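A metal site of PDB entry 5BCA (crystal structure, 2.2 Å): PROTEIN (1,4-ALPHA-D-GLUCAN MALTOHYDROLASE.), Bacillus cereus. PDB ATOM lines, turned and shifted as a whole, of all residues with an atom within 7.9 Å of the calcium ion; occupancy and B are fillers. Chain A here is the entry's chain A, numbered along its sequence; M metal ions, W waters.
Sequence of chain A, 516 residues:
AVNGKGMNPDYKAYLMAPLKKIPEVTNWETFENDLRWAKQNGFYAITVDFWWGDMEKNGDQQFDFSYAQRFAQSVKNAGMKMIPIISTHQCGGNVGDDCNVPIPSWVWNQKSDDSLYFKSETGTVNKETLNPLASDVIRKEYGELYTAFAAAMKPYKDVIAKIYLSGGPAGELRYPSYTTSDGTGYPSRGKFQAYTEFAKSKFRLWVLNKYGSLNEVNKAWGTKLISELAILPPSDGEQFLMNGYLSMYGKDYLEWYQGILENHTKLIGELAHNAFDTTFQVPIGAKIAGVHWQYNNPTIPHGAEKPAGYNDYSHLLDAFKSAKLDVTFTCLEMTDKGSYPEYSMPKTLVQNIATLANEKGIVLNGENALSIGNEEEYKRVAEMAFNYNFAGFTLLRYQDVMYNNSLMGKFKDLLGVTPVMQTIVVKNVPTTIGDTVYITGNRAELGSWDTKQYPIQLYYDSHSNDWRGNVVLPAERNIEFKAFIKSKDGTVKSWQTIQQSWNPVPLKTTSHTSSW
The side-chain carboxylate (OE2) of Glu 144 lies within salt-bridge range of the side-chain amino group (NZ) of Lys 140, 3.3 Å away. The side-chain carboxylate (OE2) of Glu 141 is in salt-bridge range of the side-chain amino group (NZ) of Lys 140 (2.4 Å). OE2 of Glu 141 is in hydrogen-bond range of NE2 of Gln 110, 2.9 Å away. O of Glu 56 is in hydrogen-bond range of NE1 of Trp 106, at 3.0 Å. The side-chain carboxylate of Glu 56 lies within hydrogen-bond range of the indole nitrogen of Trp 52 (2.6 Å). OD2 of Asp 60 is in salt-bridge range of NZ of Lys 140.
Residues that only touch the calcium ion: Lys 140 (3.99 Å). Of the 17 residues printed, 6 come within 4 Å of the calcium ion.
The calcium ion is bound by OE1 of Glu 144 (2.2 Å), OE1 of Glu 141 (2.3 Å), OE2 of Glu 56 (2.3 Å), OD1 of Asp 60 (2.4 Å), water W1 (2.5 Å) and OE1 of Gln 61 (2.6 Å).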
ATOM      1  N   TRP A  52      13.331  12.101  26.803  1.00  0.00           N
ATOM      2  CA  TRP A  52      14.643  11.537  26.935  1.00  0.00           C
ATOM      3  C   TRP A  52      15.031  10.962  25.572  1.00  0.00           C
ATOM      4  O   TRP A  52      16.130  11.240  25.063  1.00  0.00           O
ATOM      5  CB  TRP A  52      14.835  10.477  28.023  1.00  0.00           C
ATOM      6  CG  TRP A  52      16.234   9.998  28.270  1.00  0.00           C
ATOM      7  CD1 TRP A  52      17.391  10.523  27.760  1.00  0.00           C
ATOM      8  CD2 TRP A  52      16.634   8.880  29.099  1.00  0.00           C
ATOM      9  NE1 TRP A  52      18.490   9.792  28.197  1.00  0.00           N
ATOM     10  CE2 TRP A  52      18.036   8.785  29.028  1.00  0.00           C
ATOM     11  CE3 TRP A  52      15.953   7.953  29.871  1.00  0.00           C
ATOM     12  CZ2 TRP A  52      18.777   7.798  29.691  1.00  0.00           C
ATOM     13  CZ3 TRP A  52      16.678   6.962  30.528  1.00  0.00           C
ATOM     14  CH2 TRP A  52      18.085   6.871  30.443  1.00  0.00           C
ATOM     15  N   GLU A  56      18.643  12.653  23.975  1.00  0.00           N
ATOM     16  CA  GLU A  56      19.881  11.915  24.085  1.00  0.00           C
ATOM     17  C   GLU A  56      19.781  10.712  23.190  1.00  0.00           C
ATOM     18  O   GLU A  56      20.194   9.646  23.622  1.00  0.00           O
ATOM     19  CB  GLU A  56      20.186  11.458  25.511  1.00  0.00           C
ATOM     20  CG  GLU A  56      21.684  11.264  25.789  1.00  0.00           C
ATOM     21  CD  GLU A  56      21.919  10.851  27.235  1.00  0.00           C
ATOM     22  OE1 GLU A  56      20.908  10.686  27.945  1.00  0.00           O
ATOM     23  OE2 GLU A  56      23.093  10.671  27.658  1.00  0.00           O
ATOM     24  N   GLY A  59      23.374   8.652  21.465  1.00  0.00           N
ATOM     25  CA  GLY A  59      24.252   7.885  22.315  1.00  0.00           C
ATOM     26  C   GLY A  59      24.572   8.682  23.557  1.00  0.00           C
ATOM     27  O   GLY A  59      24.259   9.857  23.746  1.00  0.00           O
ATOM     28  N   ASP A  60      25.372   8.057  24.415  1.00  0.00           N
ATOM     29  CA  ASP A  60      25.688   8.646  25.688  1.00  0.00           C
ATOM     30  C   ASP A  60      26.318  10.025  25.565  1.00  0.00           C
ATOM     31  O   ASP A  60      27.395  10.268  24.976  1.00  0.00           O
ATOM     32  CB  ASP A  60      26.553   7.522  26.320  1.00  0.00           C
ATOM     33  CG  ASP A  60      26.695   7.868  27.766  1.00  0.00           C
ATOM     34  OD1 ASP A  60      25.711   8.471  28.223  1.00  0.00           O
ATOM     35  OD2 ASP A  60      27.683   7.683  28.497  1.00  0.00           O
ATOM     36  N   GLN A  61      25.704  11.037  26.194  1.00  0.00           N
ATOM     37  CA  GLN A  61      26.160  12.397  26.264  1.00  0.00           C
ATOM     38  C   GLN A  61      26.049  13.102  24.928  1.00  0.00           C
ATOM     39  O   GLN A  61      26.627  14.137  24.710  1.00  0.00           O
ATOM     40  CB  GLN A  61      27.587  12.384  26.827  1.00  0.00           C
ATOM     41  CG  GLN A  61      27.753  11.821  28.252  1.00  0.00           C
ATOM     42  CD  GLN A  61      26.900  12.522  29.307  1.00  0.00           C
ATOM     43  OE1 GLN A  61      25.763  12.120  29.544  1.00  0.00           O
ATOM     44  NE2 GLN A  61      27.333  13.572  29.996  1.00  0.00           N
ATOM     45  N   GLN A  62      25.327  12.601  23.943  1.00  0.00           N
ATOM     46  CA  GLN A  62      25.132  13.257  22.674  1.00  0.00           C
ATOM     47  C   GLN A  62      23.713  13.916  22.713  1.00  0.00           C
ATOM     48  O   GLN A  62      22.731  13.394  22.130  1.00  0.00           O
ATOM     49  CB  GLN A  62      25.093  12.245  21.537  1.00  0.00           C
ATOM     50  CG  GLN A  62      26.250  11.280  21.787  1.00  0.00           C
ATOM     51  CD  GLN A  62      26.651  10.649  20.473  1.00  0.00           C
ATOM     52  OE1 GLN A  62      26.230  11.217  19.506  1.00  0.00           O
ATOM     53  NE2 GLN A  62      27.387   9.568  20.620  1.00  0.00           N
ATOM     54  N   PHE A  63      23.701  15.010  23.431  1.00  0.00           N
ATOM     55  CA  PHE A  63      22.550  15.790  23.763  1.00  0.00           C
ATOM     56  C   PHE A  63      22.073  16.706  22.663  1.00  0.00           C
ATOM     57  O   PHE A  63      22.761  17.002  21.701  1.00  0.00           O
ATOM     58  CB  PHE A  63      22.917  16.656  24.971  1.00  0.00           C
ATOM     59  CG  PHE A  63      23.147  15.849  26.200  1.00  0.00           C
ATOM     60  CD1 PHE A  63      22.150  15.028  26.707  1.00  0.00           C
ATOM     61  CD2 PHE A  63      24.349  15.906  26.880  1.00  0.00           C
ATOM     62  CE1 PHE A  63      22.328  14.327  27.887  1.00  0.00           C
ATOM     63  CE2 PHE A  63      24.522  15.178  28.028  1.00  0.00           C
ATOM     64  CZ  PHE A  63      23.544  14.368  28.559  1.00  0.00           C
ATOM     65  N   TRP A 106      20.246   2.741  23.001  1.00  0.00           N
ATOM     66  CA  TRP A 106      21.549   2.310  23.455  1.00  0.00           C
ATOM     67  C   TRP A 106      21.641   2.062  24.957  1.00  0.00           C
ATOM     68  O   TRP A 106      22.597   1.468  25.504  1.00  0.00           O
ATOM     69  CB  TRP A 106      22.673   3.362  23.058  1.00  0.00           C
ATOM     70  CG  TRP A 106      22.276   4.757  23.446  1.00  0.00           C
ATOM     71  CD1 TRP A 106      21.601   5.705  22.708  1.00  0.00           C
ATOM     72  CD2 TRP A 106      22.535   5.356  24.726  1.00  0.00           C
ATOM     73  NE1 TRP A 106      21.430   6.863  23.479  1.00  0.00           N
ATOM     74  CE2 TRP A 106      21.998   6.634  24.740  1.00  0.00           C
ATOM     75  CE3 TRP A 106      23.167   4.891  25.885  1.00  0.00           C
ATOM     76  CZ2 TRP A 106      22.043   7.442  25.849  1.00  0.00           C
ATOM     77  CZ3 TRP A 106      23.230   5.676  27.009  1.00  0.00           C
ATOM     78  CH2 TRP A 106      22.635   6.906  26.944  1.00  0.00           C
ATOM     79  N   VAL A 107      20.680   2.613  25.708  1.00  0.00           N
ATOM     80  CA  VAL A 107      20.726   2.463  27.185  1.00  0.00           C
ATOM     81  C   VAL A 107      20.631   0.992  27.580  1.00  0.00           C
ATOM     82  O   VAL A 107      21.195   0.520  28.560  1.00  0.00           O
ATOM     83  CB  VAL A 107      19.592   3.252  27.834  1.00  0.00           C
ATOM     84  CG1 VAL A 107      19.655   3.189  29.342  1.00  0.00           C
ATOM     85  CG2 VAL A 107      19.710   4.715  27.406  1.00  0.00           C
ATOM     86  N   GLN A 110      23.746  -1.095  28.093  1.00  0.00           N
ATOM     87  CA  GLN A 110      24.557  -0.844  29.289  1.00  0.00           C
ATOM     88  C   GLN A 110      24.654  -2.055  30.201  1.00  0.00           C
ATOM     89  O   GLN A 110      25.468  -2.083  31.138  1.00  0.00           O
ATOM     90  CB  GLN A 110      24.015   0.420  29.977  1.00  0.00           C
ATOM     91  CG  GLN A 110      24.901   1.669  29.699  1.00  0.00           C
ATOM     92  CD  GLN A 110      24.535   2.824  30.606  1.00  0.00           C
ATOM     93  OE1 GLN A 110      24.826   2.979  31.820  1.00  0.00           O
ATOM     94  NE2 GLN A 110      23.780   3.753  29.999  1.00  0.00           N
ATOM     95  N   VAL A 137      22.726   2.620  37.115  1.00  0.00           N
ATOM     96  CA  VAL A 137      22.431   3.116  35.782  1.00  0.00           C
ATOM     97  C   VAL A 137      21.507   4.323  35.865  1.00  0.00           C
ATOM     98  O   VAL A 137      21.752   5.291  35.132  1.00  0.00           O
ATOM     99  CB  VAL A 137      21.762   2.102  34.879  1.00  0.00           C
ATOM    100  CG1 VAL A 137      21.288   2.661  33.537  1.00  0.00           C
ATOM    101  CG2 VAL A 137      22.695   0.912  34.572  1.00  0.00           C
ATOM    102  N   LYS A 140      23.673   7.493  37.226  1.00  0.00           N
ATOM    103  CA  LYS A 140      24.508   8.039  36.168  1.00  0.00           C
ATOM    104  C   LYS A 140      23.693   8.780  35.100  1.00  0.00           C
ATOM    105  O   LYS A 140      23.930   9.965  34.854  1.00  0.00           O
ATOM    106  CB  LYS A 140      25.349   6.961  35.431  1.00  0.00           C
ATOM    107  CG  LYS A 140      25.758   7.149  33.991  1.00  0.00           C
ATOM    108  CD  LYS A 140      26.586   5.988  33.372  1.00  0.00           C
ATOM    109  CE  LYS A 140      27.467   6.518  32.225  1.00  0.00           C
ATOM    110  NZ  LYS A 140      26.693   7.231  31.169  1.00  0.00           N
ATOM    111  N   GLU A 141      22.836   8.047  34.373  1.00  0.00           N
ATOM    112  CA  GLU A 141      22.057   8.593  33.290  1.00  0.00           C
ATOM    113  C   GLU A 141      21.090   9.707  33.587  1.00  0.00           C
ATOM    114  O   GLU A 141      21.011  10.683  32.797  1.00  0.00           O
ATOM    115  CB  GLU A 141      21.331   7.507  32.510  1.00  0.00           C
ATOM    116  CG  GLU A 141      22.295   6.430  32.007  1.00  0.00           C
ATOM    117  CD  GLU A 141      23.404   7.100  31.176  1.00  0.00           C
ATOM    118  OE1 GLU A 141      23.260   8.231  30.657  1.00  0.00           O
ATOM    119  OE2 GLU A 141      24.401   6.385  31.013  1.00  0.00           O
ATOM    120  N   TYR A 142      20.463   9.683  34.765  1.00  0.00           N
ATOM    121  CA  TYR A 142      19.538  10.772  35.084  1.00  0.00           C
ATOM    122  C   TYR A 142      20.378  11.867  35.688  1.00  0.00           C
ATOM    123  O   TYR A 142      19.945  13.003  35.548  1.00  0.00           O
ATOM    124  CB  TYR A 142      18.477  10.336  36.061  1.00  0.00           C
ATOM    125  CG  TYR A 142      17.345   9.435  35.728  1.00  0.00           C
ATOM    126  CD1 TYR A 142      17.391   8.553  34.680  1.00  0.00           C
ATOM    127  CD2 TYR A 142      16.168   9.468  36.488  1.00  0.00           C
ATOM    128  CE1 TYR A 142      16.346   7.712  34.362  1.00  0.00           C
ATOM    129  CE2 TYR A 142      15.104   8.628  36.249  1.00  0.00           C
ATOM    130  CZ  TYR A 142      15.204   7.749  35.189  1.00  0.00           C
ATOM    131  OH  TYR A 142      14.185   6.906  34.856  1.00  0.00           O
ATOM    132  N   GLY A 143      21.417  11.527  36.453  1.00  0.00           N
ATOM    133  CA  GLY A 143      22.190  12.694  37.002  1.00  0.00           C
ATOM    134  C   GLY A 143      22.754  13.474  35.754  1.00  0.00           C
ATOM    135  O   GLY A 143      22.737  14.700  35.684  1.00  0.00           O
ATOM    136  N   GLU A 144      23.284  12.779  34.750  1.00  0.00           N
ATOM    137  CA  GLU A 144      23.849  13.458  33.582  1.00  0.00           C
ATOM    138  C   GLU A 144      22.809  14.255  32.797  1.00  0.00           C
ATOM    139  O   GLU A 144      23.115  15.319  32.267  1.00  0.00           O
ATOM    140  CB  GLU A 144      24.403  12.410  32.567  1.00  0.00           C
ATOM    141  CG  GLU A 144      25.712  11.821  33.108  1.00  0.00           C
ATOM    142  CD  GLU A 144      26.087  10.588  32.258  1.00  0.00           C
ATOM    143  OE1 GLU A 144      25.351  10.114  31.384  1.00  0.00           O
ATOM    144  OE2 GLU A 144      27.273  10.256  32.463  1.00  0.00           O
ATOM    145  N   LEU A 145      21.641  13.646  32.638  1.00  0.00           N
ATOM    146  CA  LEU A 145      20.567  14.242  31.844  1.00  0.00           C
ATOM    147  C   LEU A 145      20.015  15.452  32.575  1.00  0.00           C
ATOM    148  O   LEU A 145      20.035  16.561  32.042  1.00  0.00           O
ATOM    149  CB  LEU A 145      19.484  13.253  31.477  1.00  0.00           C
ATOM    150  CG  LEU A 145      18.264  13.790  30.765  1.00  0.00           C
ATOM    151  CD1 LEU A 145      18.501  13.935  29.256  1.00  0.00           C
ATOM    152  CD2 LEU A 145      17.050  12.908  30.959  1.00  0.00           C
HETATM  153 CA    CA M   1      24.293   9.947  29.507  1.00  0.00          CA
HETATM  154  O   HOH W   1      22.002  10.791  30.009  1.00  0.00           O
